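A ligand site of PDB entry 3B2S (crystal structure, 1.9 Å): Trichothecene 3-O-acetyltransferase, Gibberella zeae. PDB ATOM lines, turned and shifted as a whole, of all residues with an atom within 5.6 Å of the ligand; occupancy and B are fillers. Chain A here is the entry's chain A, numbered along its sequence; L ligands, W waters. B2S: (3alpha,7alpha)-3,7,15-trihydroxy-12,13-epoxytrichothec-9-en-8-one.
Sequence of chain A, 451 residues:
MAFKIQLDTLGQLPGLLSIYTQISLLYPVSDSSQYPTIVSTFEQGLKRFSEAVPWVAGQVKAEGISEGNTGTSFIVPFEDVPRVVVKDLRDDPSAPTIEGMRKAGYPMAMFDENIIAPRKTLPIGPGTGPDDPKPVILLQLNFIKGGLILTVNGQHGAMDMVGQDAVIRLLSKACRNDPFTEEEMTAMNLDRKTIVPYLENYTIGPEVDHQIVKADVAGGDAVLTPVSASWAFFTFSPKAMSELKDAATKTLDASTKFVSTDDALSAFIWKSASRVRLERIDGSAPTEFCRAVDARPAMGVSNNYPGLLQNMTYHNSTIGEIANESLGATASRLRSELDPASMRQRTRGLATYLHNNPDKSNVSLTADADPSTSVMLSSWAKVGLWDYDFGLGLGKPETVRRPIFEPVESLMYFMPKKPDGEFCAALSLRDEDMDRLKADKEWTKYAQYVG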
ATOM      1  N   GLY A  15     -28.817  18.386  26.356  1.00  0.00           N
ATOM      2  CA  GLY A  15     -28.108  18.153  25.101  1.00  0.00           C
ATOM      3  C   GLY A  15     -26.600  18.289  25.209  1.00  0.00           C
ATOM      4  O   GLY A  15     -25.865  17.724  24.400  1.00  0.00           O
ATOM      5  N   LEU A  16     -26.138  19.036  26.207  1.00  0.00           N
ATOM      6  CA  LEU A  16     -24.703  19.204  26.467  1.00  0.00           C
ATOM      7  C   LEU A  16     -24.144  18.136  27.409  1.00  0.00           C
ATOM      8  O   LEU A  16     -23.036  17.601  27.191  1.00  0.00           O
ATOM      9  CB  LEU A  16     -24.421  20.594  27.002  1.00  0.00           C
ATOM     10  CG  LEU A  16     -24.840  21.701  26.024  1.00  0.00           C
ATOM     11  CD1 LEU A  16     -24.316  23.032  26.527  1.00  0.00           C
ATOM     12  CD2 LEU A  16     -24.323  21.425  24.619  1.00  0.00           C
ATOM     13  N   ILE A  19     -23.013  14.659  25.529  1.00  0.00           N
ATOM     14  CA  ILE A  19     -22.115  14.568  24.389  1.00  0.00           C
ATOM     15  C   ILE A  19     -20.648  14.930  24.735  1.00  0.00           C
ATOM     16  O   ILE A  19     -20.393  15.622  25.734  1.00  0.00           O
ATOM     17  CB  ILE A  19     -22.619  15.411  23.198  1.00  0.00           C
ATOM     18  CG1 ILE A  19     -22.637  16.900  23.531  1.00  0.00           C
ATOM     19  CG2 ILE A  19     -24.038  14.959  22.752  1.00  0.00           C
ATOM     20  CD1 ILE A  19     -22.879  17.782  22.321  1.00  0.00           C
ATOM     21  N   THR A  21     -17.254  16.732  22.890  1.00  0.00           N
ATOM     22  CA  THR A  21     -16.641  17.467  21.782  1.00  0.00           C
ATOM     23  C   THR A  21     -15.251  16.888  21.488  1.00  0.00           C
ATOM     24  O   THR A  21     -14.425  16.765  22.402  1.00  0.00           O
ATOM     25  CB  THR A  21     -16.507  18.955  22.127  1.00  0.00           C
ATOM     26  OG1 THR A  21     -17.793  19.456  22.476  1.00  0.00           O
ATOM     27  CG2 THR A  21     -15.932  19.738  20.925  1.00  0.00           C
ATOM     28  N   THR A 121     -18.674  10.807  20.133  1.00  0.00           N
ATOM     29  CA  THR A 121     -19.311  12.100  20.360  1.00  0.00           C
ATOM     30  C   THR A 121     -20.684  11.912  21.030  1.00  0.00           C
ATOM     31  O   THR A 121     -21.037  12.565  22.030  1.00  0.00           O
ATOM     32  CB  THR A 121     -19.505  12.830  19.006  1.00  0.00           C
ATOM     33  OG1 THR A 121     -18.229  13.132  18.444  1.00  0.00           O
ATOM     34  CG2 THR A 121     -20.333  14.134  19.175  1.00  0.00           C
ATOM     35  N   LEU A 122     -21.464  11.012  20.456  1.00  0.00           N
ATOM     36  CA  LEU A 122     -22.838  10.834  20.884  1.00  0.00           C
ATOM     37  C   LEU A 122     -22.902   9.676  21.887  1.00  0.00           C
ATOM     38  O   LEU A 122     -22.037   8.817  21.885  1.00  0.00           O
ATOM     39  CB  LEU A 122     -23.724  10.554  19.657  1.00  0.00           C
ATOM     40  CG  LEU A 122     -23.777  11.670  18.586  1.00  0.00           C
ATOM     41  CD1 LEU A 122     -24.655  11.225  17.420  1.00  0.00           C
ATOM     42  CD2 LEU A 122     -24.269  12.985  19.169  1.00  0.00           C
ATOM     43  N   HIS A 156     -19.121  17.855  27.299  1.00  0.00           N
ATOM     44  CA  HIS A 156     -19.704  19.123  26.863  1.00  0.00           C
ATOM     45  C   HIS A 156     -20.410  19.959  27.944  1.00  0.00           C
ATOM     46  O   HIS A 156     -20.464  21.141  27.844  1.00  0.00           O
ATOM     47  CB  HIS A 156     -20.513  19.006  25.573  1.00  0.00           C
ATOM     48  CG  HIS A 156     -20.604  20.274  24.786  1.00  0.00           C
ATOM     49  ND1 HIS A 156     -20.580  21.518  25.355  1.00  0.00           N
ATOM     50  CD2 HIS A 156     -20.749  20.484  23.462  1.00  0.00           C
ATOM     51  CE1 HIS A 156     -20.701  22.440  24.424  1.00  0.00           C
ATOM     52  NE2 HIS A 156     -20.793  21.840  23.268  1.00  0.00           N
ATOM     53  N   ASP A 221     -32.341  18.240  20.329  1.00  0.00           N
ATOM     54  CA  ASP A 221     -30.880  18.026  20.396  1.00  0.00           C
ATOM     55  C   ASP A 221     -30.411  16.889  19.501  1.00  0.00           C
ATOM     56  O   ASP A 221     -31.000  15.816  19.501  1.00  0.00           O
ATOM     57  CB  ASP A 221     -30.436  17.756  21.843  1.00  0.00           C
ATOM     58  CG  ASP A 221     -30.692  18.933  22.775  1.00  0.00           C
ATOM     59  OD1 ASP A 221     -30.378  20.096  22.418  1.00  0.00           O
ATOM     60  OD2 ASP A 221     -31.194  18.696  23.882  1.00  0.00           O
ATOM     61  N   ALA A 222     -29.339  17.143  18.739  1.00  0.00           N
ATOM     62  CA  ALA A 222     -28.669  16.145  17.876  1.00  0.00           C
ATOM     63  C   ALA A 222     -29.654  15.179  17.224  1.00  0.00           C
ATOM     64  O   ALA A 222     -29.586  13.943  17.410  1.00  0.00           O
ATOM     65  CB  ALA A 222     -27.582  15.392  18.669  1.00  0.00           C
ATOM     66  N   VAL A 223     -30.587  15.768  16.465  1.00  0.00           N
ATOM     67  CA  VAL A 223     -31.625  14.990  15.787  1.00  0.00           C
ATOM     68  C   VAL A 223     -30.996  14.203  14.637  1.00  0.00           C
ATOM     69  O   VAL A 223     -30.432  14.784  13.699  1.00  0.00           O
ATOM     70  CB  VAL A 223     -32.792  15.897  15.283  1.00  0.00           C
ATOM     71  CG1 VAL A 223     -33.922  15.058  14.633  1.00  0.00           C
ATOM     72  CG2 VAL A 223     -33.331  16.793  16.438  1.00  0.00           C
ATOM     73  N   ALA A 292     -23.638  29.466  17.016  1.00  0.00           N
ATOM     74  CA  ALA A 292     -23.055  29.406  18.375  1.00  0.00           C
ATOM     75  C   ALA A 292     -22.161  30.627  18.607  1.00  0.00           C
ATOM     76  O   ALA A 292     -21.430  31.059  17.683  1.00  0.00           O
ATOM     77  CB  ALA A 292     -22.243  28.094  18.600  1.00  0.00           C
ATOM     78  N   GLN A 310     -21.660  29.615  26.626  1.00  0.00           N
ATOM     79  CA  GLN A 310     -21.916  29.714  25.190  1.00  0.00           C
ATOM     80  C   GLN A 310     -23.424  29.883  25.045  1.00  0.00           C
ATOM     81  O   GLN A 310     -24.192  29.379  25.870  1.00  0.00           O
ATOM     82  CB  GLN A 310     -21.497  28.398  24.534  1.00  0.00           C
ATOM     83  CG  GLN A 310     -21.438  28.416  23.015  1.00  0.00           C
ATOM     84  CD  GLN A 310     -21.903  27.101  22.415  1.00  0.00           C
ATOM     85  OE1 GLN A 310     -21.265  26.060  22.593  1.00  0.00           O
ATOM     86  NE2 GLN A 310     -23.041  27.150  21.717  1.00  0.00           N
ATOM     87  N   MET A 312     -26.489  30.866  21.576  1.00  0.00           N
ATOM     88  CA  MET A 312     -26.684  30.913  20.129  1.00  0.00           C
ATOM     89  C   MET A 312     -27.317  32.258  19.784  1.00  0.00           C
ATOM     90  O   MET A 312     -27.907  32.920  20.641  1.00  0.00           O
ATOM     91  CB  MET A 312     -27.670  29.833  19.683  1.00  0.00           C
ATOM     92  CG  MET A 312     -27.402  28.440  20.211  1.00  0.00           C
ATOM     93  SD  MET A 312     -25.921  27.674  19.555  1.00  0.00           S
ATOM     94  CE  MET A 312     -26.494  27.185  17.917  1.00  0.00           C
ATOM     95  N   LEU A 365     -30.579  24.404  22.945  1.00  0.00           N
ATOM     96  CA  LEU A 365     -30.036  25.437  22.051  1.00  0.00           C
ATOM     97  C   LEU A 365     -30.538  25.342  20.584  1.00  0.00           C
ATOM     98  O   LEU A 365     -30.335  26.280  19.796  1.00  0.00           O
ATOM     99  CB  LEU A 365     -28.515  25.378  22.088  1.00  0.00           C
ATOM    100  CG  LEU A 365     -27.848  25.755  23.417  1.00  0.00           C
ATOM    101  CD1 LEU A 365     -26.336  25.718  23.254  1.00  0.00           C
ATOM    102  CD2 LEU A 365     -28.277  27.141  23.915  1.00  0.00           C
ATOM    103  N   THR A 366     -31.146  24.215  20.211  1.00  0.00           N
ATOM    104  CA  THR A 366     -31.727  24.054  18.882  1.00  0.00           C
ATOM    105  C   THR A 366     -33.177  23.522  19.020  1.00  0.00           C
ATOM    106  O   THR A 366     -33.632  22.681  18.239  1.00  0.00           O
ATOM    107  CB  THR A 366     -30.881  23.127  17.981  1.00  0.00           C
ATOM    108  OG1 THR A 366     -30.697  21.880  18.648  1.00  0.00           O
ATOM    109  CG2 THR A 366     -29.472  23.722  17.719  1.00  0.00           C
ATOM    110  N   MET A 376     -27.331  24.764  11.715  1.00  0.00           N
ATOM    111  CA  MET A 376     -26.861  24.857  13.094  1.00  0.00           C
ATOM    112  C   MET A 376     -25.322  24.829  13.040  1.00  0.00           C
ATOM    113  O   MET A 376     -24.730  23.778  12.840  1.00  0.00           O
ATOM    114  CB  MET A 376     -27.401  23.698  13.942  1.00  0.00           C
ATOM    115  CG  MET A 376     -28.950  23.653  14.054  1.00  0.00           C
ATOM    116  SD  MET A 376     -29.624  22.071  14.626  1.00  0.00           S
ATOM    117  CE  MET A 376     -29.091  21.005  13.303  1.00  0.00           C
ATOM    118  N   LEU A 377     -24.703  26.001  13.192  1.00  0.00           N
ATOM    119  CA  LEU A 377     -23.282  26.142  12.937  1.00  0.00           C
ATOM    120  C   LEU A 377     -22.548  26.618  14.193  1.00  0.00           C
ATOM    121  O   LEU A 377     -22.989  27.545  14.853  1.00  0.00           O
ATOM    122  CB  LEU A 377     -23.036  27.183  11.817  1.00  0.00           C
ATOM    123  CG  LEU A 377     -21.563  27.682  11.765  1.00  0.00           C
ATOM    124  CD1 LEU A 377     -20.736  26.662  11.084  1.00  0.00           C
ATOM    125  CD2 LEU A 377     -21.406  29.001  11.061  1.00  0.00           C
ATOM    126  N   SER A 378     -21.439  25.963  14.493  1.00  0.00           N
ATOM    127  CA  SER A 378     -20.538  26.419  15.546  1.00  0.00           C
ATOM    128  C   SER A 378     -19.137  26.659  14.976  1.00  0.00           C
ATOM    129  O   SER A 378     -18.471  25.714  14.530  1.00  0.00           O
ATOM    130  CB  SER A 378     -20.455  25.392  16.668  1.00  0.00           C
ATOM    131  OG  SER A 378     -19.703  25.967  17.754  1.00  0.00           O
ATOM    132  N   TRP A 380     -15.324  27.281  15.365  1.00  0.00           N
ATOM    133  CA  TRP A 380     -14.146  27.173  16.238  1.00  0.00           C
ATOM    134  C   TRP A 380     -12.992  27.975  15.693  1.00  0.00           C
ATOM    135  O   TRP A 380     -11.840  27.768  16.080  1.00  0.00           O
ATOM    136  CB  TRP A 380     -13.721  25.697  16.381  1.00  0.00           C
ATOM    137  CG  TRP A 380     -14.793  24.806  16.931  1.00  0.00           C
ATOM    138  CD1 TRP A 380     -15.890  25.206  17.635  1.00  0.00           C
ATOM    139  CD2 TRP A 380     -14.847  23.373  16.871  1.00  0.00           C
ATOM    140  NE1 TRP A 380     -16.641  24.104  18.017  1.00  0.00           N
ATOM    141  CE2 TRP A 380     -16.019  22.970  17.557  1.00  0.00           C
ATOM    142  CE3 TRP A 380     -14.027  22.384  16.304  1.00  0.00           C
ATOM    143  CZ2 TRP A 380     -16.403  21.614  17.691  1.00  0.00           C
ATOM    144  CZ3 TRP A 380     -14.397  21.042  16.427  1.00  0.00           C
ATOM    145  CH2 TRP A 380     -15.574  20.674  17.125  1.00  0.00           C
ATOM    146  N   PHE A 405     -18.319  11.613  12.768  1.00  0.00           N
ATOM    147  CA  PHE A 405     -19.220  10.811  13.585  1.00  0.00           C
ATOM    148  C   PHE A 405     -20.534  10.630  12.796  1.00  0.00           C
ATOM    149  O   PHE A 405     -20.546  10.837  11.577  1.00  0.00           O
ATOM    150  CB  PHE A 405     -19.395  11.383  15.013  1.00  0.00           C
ATOM    151  CG  PHE A 405     -20.053  12.746  15.105  1.00  0.00           C
ATOM    152  CD1 PHE A 405     -21.349  12.858  15.608  1.00  0.00           C
ATOM    153  CD2 PHE A 405     -19.367  13.907  14.754  1.00  0.00           C
ATOM    154  CE1 PHE A 405     -21.980  14.120  15.712  1.00  0.00           C
ATOM    155  CE2 PHE A 405     -19.962  15.160  14.864  1.00  0.00           C
ATOM    156  CZ  PHE A 405     -21.288  15.274  15.360  1.00  0.00           C
ATOM    157  N   VAL A 408     -25.452  14.450  11.495  1.00  0.00           N
ATOM    158  CA  VAL A 408     -26.555  15.135  12.173  1.00  0.00           C
ATOM    159  C   VAL A 408     -27.020  16.216  11.180  1.00  0.00           C
ATOM    160  O   VAL A 408     -26.339  17.202  10.962  1.00  0.00           O
ATOM    161  CB  VAL A 408     -26.099  15.769  13.509  1.00  0.00           C
ATOM    162  CG1 VAL A 408     -27.249  16.519  14.195  1.00  0.00           C
ATOM    163  CG2 VAL A 408     -25.535  14.694  14.430  1.00  0.00           C
ATOM    164  N   LEU A 411     -26.119  20.212  10.904  1.00  0.00           N
ATOM    165  CA  LEU A 411     -25.065  20.596  11.835  1.00  0.00           C
ATOM    166  C   LEU A 411     -23.787  20.878  11.060  1.00  0.00           C
ATOM    167  O   LEU A 411     -23.436  20.159  10.117  1.00  0.00           O
ATOM    168  CB  LEU A 411     -24.854  19.468  12.866  1.00  0.00           C
ATOM    169  CG  LEU A 411     -23.819  19.682  13.982  1.00  0.00           C
ATOM    170  CD1 LEU A 411     -24.234  20.867  14.893  1.00  0.00           C
ATOM    171  CD2 LEU A 411     -23.712  18.397  14.797  1.00  0.00           C
ATOM    172  N   MET A 412     -23.075  21.928  11.487  1.00  0.00           N
ATOM    173  CA  MET A 412     -21.887  22.402  10.792  1.00  0.00           C
ATOM    174  C   MET A 412     -20.903  23.028  11.772  1.00  0.00           C
ATOM    175  O   MET A 412     -21.322  23.520  12.813  1.00  0.00           O
ATOM    176  CB  MET A 412     -22.289  23.474   9.791  1.00  0.00           C
ATOM    177  CG  MET A 412     -23.359  23.014   8.809  1.00  0.00           C
ATOM    178  SD  MET A 412     -23.591  24.280   7.565  1.00  0.00           S
ATOM    179  CE  MET A 412     -24.952  23.496   6.693  1.00  0.00           C
ATOM    180  N   TYR A 413     -19.614  22.966  11.434  1.00  0.00           N
ATOM    181  CA  TYR A 413     -18.539  23.581  12.231  1.00  0.00           C
ATOM    182  C   TYR A 413     -17.544  24.319  11.330  1.00  0.00           C
ATOM    183  O   TYR A 413     -17.332  23.910  10.207  1.00  0.00           O
ATOM    184  CB  TYR A 413     -17.749  22.482  12.973  1.00  0.00           C
ATOM    185  CG  TYR A 413     -18.588  21.685  13.943  1.00  0.00           C
ATOM    186  CD1 TYR A 413     -19.089  20.416  13.612  1.00  0.00           C
ATOM    187  CD2 TYR A 413     -18.871  22.211  15.202  1.00  0.00           C
ATOM    188  CE1 TYR A 413     -19.861  19.704  14.518  1.00  0.00           C
ATOM    189  CE2 TYR A 413     -19.642  21.498  16.118  1.00  0.00           C
ATOM    190  CZ  TYR A 413     -20.130  20.258  15.776  1.00  0.00           C
ATOM    191  OH  TYR A 413     -20.896  19.600  16.714  1.00  0.00           O
HETATM  192  C13 B2S L   1     -24.403  23.592  17.178  1.00  0.00           C
HETATM  193  O2  B2S L   1     -23.969  24.646  18.132  1.00  0.00           O
HETATM  194  C12 B2S L   1     -23.702  23.253  18.479  1.00  0.00           C
HETATM  195  C5  B2S L   1     -24.382  22.691  19.744  1.00  0.00           C
HETATM  196  C14 B2S L   1     -25.727  23.373  20.078  1.00  0.00           C
HETATM  197  C4  B2S L   1     -23.279  23.090  20.780  1.00  0.00           C
HETATM  198  C3  B2S L   1     -21.984  23.380  19.963  1.00  0.00           C
HETATM  199  O3  B2S L   1     -20.832  22.666  20.458  1.00  0.00           O
HETATM  200  C2  B2S L   1     -22.268  22.849  18.551  1.00  0.00           C
HETATM  201  O1  B2S L   1     -22.059  21.387  18.559  1.00  0.00           O
HETATM  202  C11 B2S L   1     -23.209  20.527  18.979  1.00  0.00           C
HETATM  203  C10 B2S L   1     -22.907  19.135  19.080  1.00  0.00           C
HETATM  204  C9  B2S L   1     -24.011  18.363  18.682  1.00  0.00           C
HETATM  205  C16 B2S L   1     -23.923  16.838  18.652  1.00  0.00           C
HETATM  206  C8  B2S L   1     -25.218  19.031  18.344  1.00  0.00           C
HETATM  207  O5  B2S L   1     -26.223  18.393  18.011  1.00  0.00           O
HETATM  208  C7  B2S L   1     -25.294  20.604  18.396  1.00  0.00           C
HETATM  209  O4  B2S L   1     -26.637  21.122  18.389  1.00  0.00           O
HETATM  210  C6  B2S L   1     -24.485  21.143  19.614  1.00  0.00           C
HETATM  211  C15 B2S L   1     -24.956  20.464  20.930  1.00  0.00           C
HETATM  212  O6  B2S L   1     -26.070  19.604  20.600  1.00  0.00           O
HETATM  213  O   HOH W   1     -28.766  19.486  17.327  1.00  0.00           O
HETATM  214  O   HOH W   2     -19.283  20.301  20.042  1.00  0.00           O
HETATM  215  O   HOH W   3     -18.965  24.294  19.594  1.00  0.00           O
HETATM  216  O   HOH W   4     -28.593  21.353  20.821  1.00  0.00           O
HETATM  217  O   HOH W   5     -26.769  17.295  21.836  1.00  0.00           O
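O1 of the ligand lies within hydrogen-bond range of OH of Tyr 413, at 2.8 Å. A ring nitrogen (NE2) of His 156 sits at hydrogen-bond distance from an oxygen (O3) of the ligand. O5 of the ligand sits close to N of Ala 222.
The backbone NH of His 156 is in hydrogen-bond range of the backbone carbonyl oxygen of Ile 19, 3.0 Å away. The side-chain sulfur (SD) of Met 312 lies within hydrogen-bond range of the side-chain amide nitrogen (NE2) of Gln 310 (3.6 Å). The backbone carbonyl oxygen (O) of Met 412 is in hydrogen-bond range of the backbone NH (N) of Ser 378, at 3.0 Å. O of Leu 377 lies within hydrogen-bond range of N of Ala 292.
Leu 16 touches the ligand (CD2 to C15, 3.9 Å). CD1 of Ile 19 touches C10 of the ligand, 3.5 Å away. CD2 of Leu 122 touches C16 of the ligand, 3.9 Å away. Ala 292 touches the ligand. Gln 310 touches the ligand (OE1 to C3, 3.8 Å). CE of Met 312 touches O2 of the ligand, at 3.6 Å. CB of Leu 365 touches C14 of the ligand, 3.98 Å away. Thr 366 touches the ligand. Ser 378 touches the ligand (CB to C2, 3.6 Å). Leu 411 touches the ligand. Hydrophobic or aromatic side chains that line the ligand: Leu 16, Ile 19, Leu 122, His 156, Ala 222, Ala 292, Met 312, Leu 365, Leu 411 and Tyr 413. 13 residues have an atom within 4 Å of the ligand: Leu 16, Ile 19, Leu 122, His 156, Ala 222, Ala 292, Gln 310, Met 312, Leu 365, Thr 366, Ser 378, Leu 411 and Tyr 413.
Water W3 lies within hydrogen-bond range of the side-chain hydroxyl (OG) of Ser 378 (2.6 Å), an oxygen (O3) of the ligand (2.6 Å) and the indole nitrogen (NE1) of Trp 380 (2.8 Å). Water W5 lies within hydrogen-bond range of O6 of the ligand (2.7 Å) and O of Gly 15 (2.8 Å). Water W1 lies within hydrogen-bond range of N of Ala 222 (2.8 Å), O5 of the ligand (2.9 Å) and OG1 of Thr 366 (3.3 Å). Water W2 bridges an oxygen (O3) of the ligand (2.9 Å) and the side-chain hydroxyl (OG1) of Thr 21 (3.0 Å). Water W4 lies within hydrogen-bond range of the side-chain carboxylate of Asp 221 (2.7 Å), the side-chain hydroxyl of Thr 366 (3.1 Å) and an oxygen (O6) of the ligand (3.1 Å).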
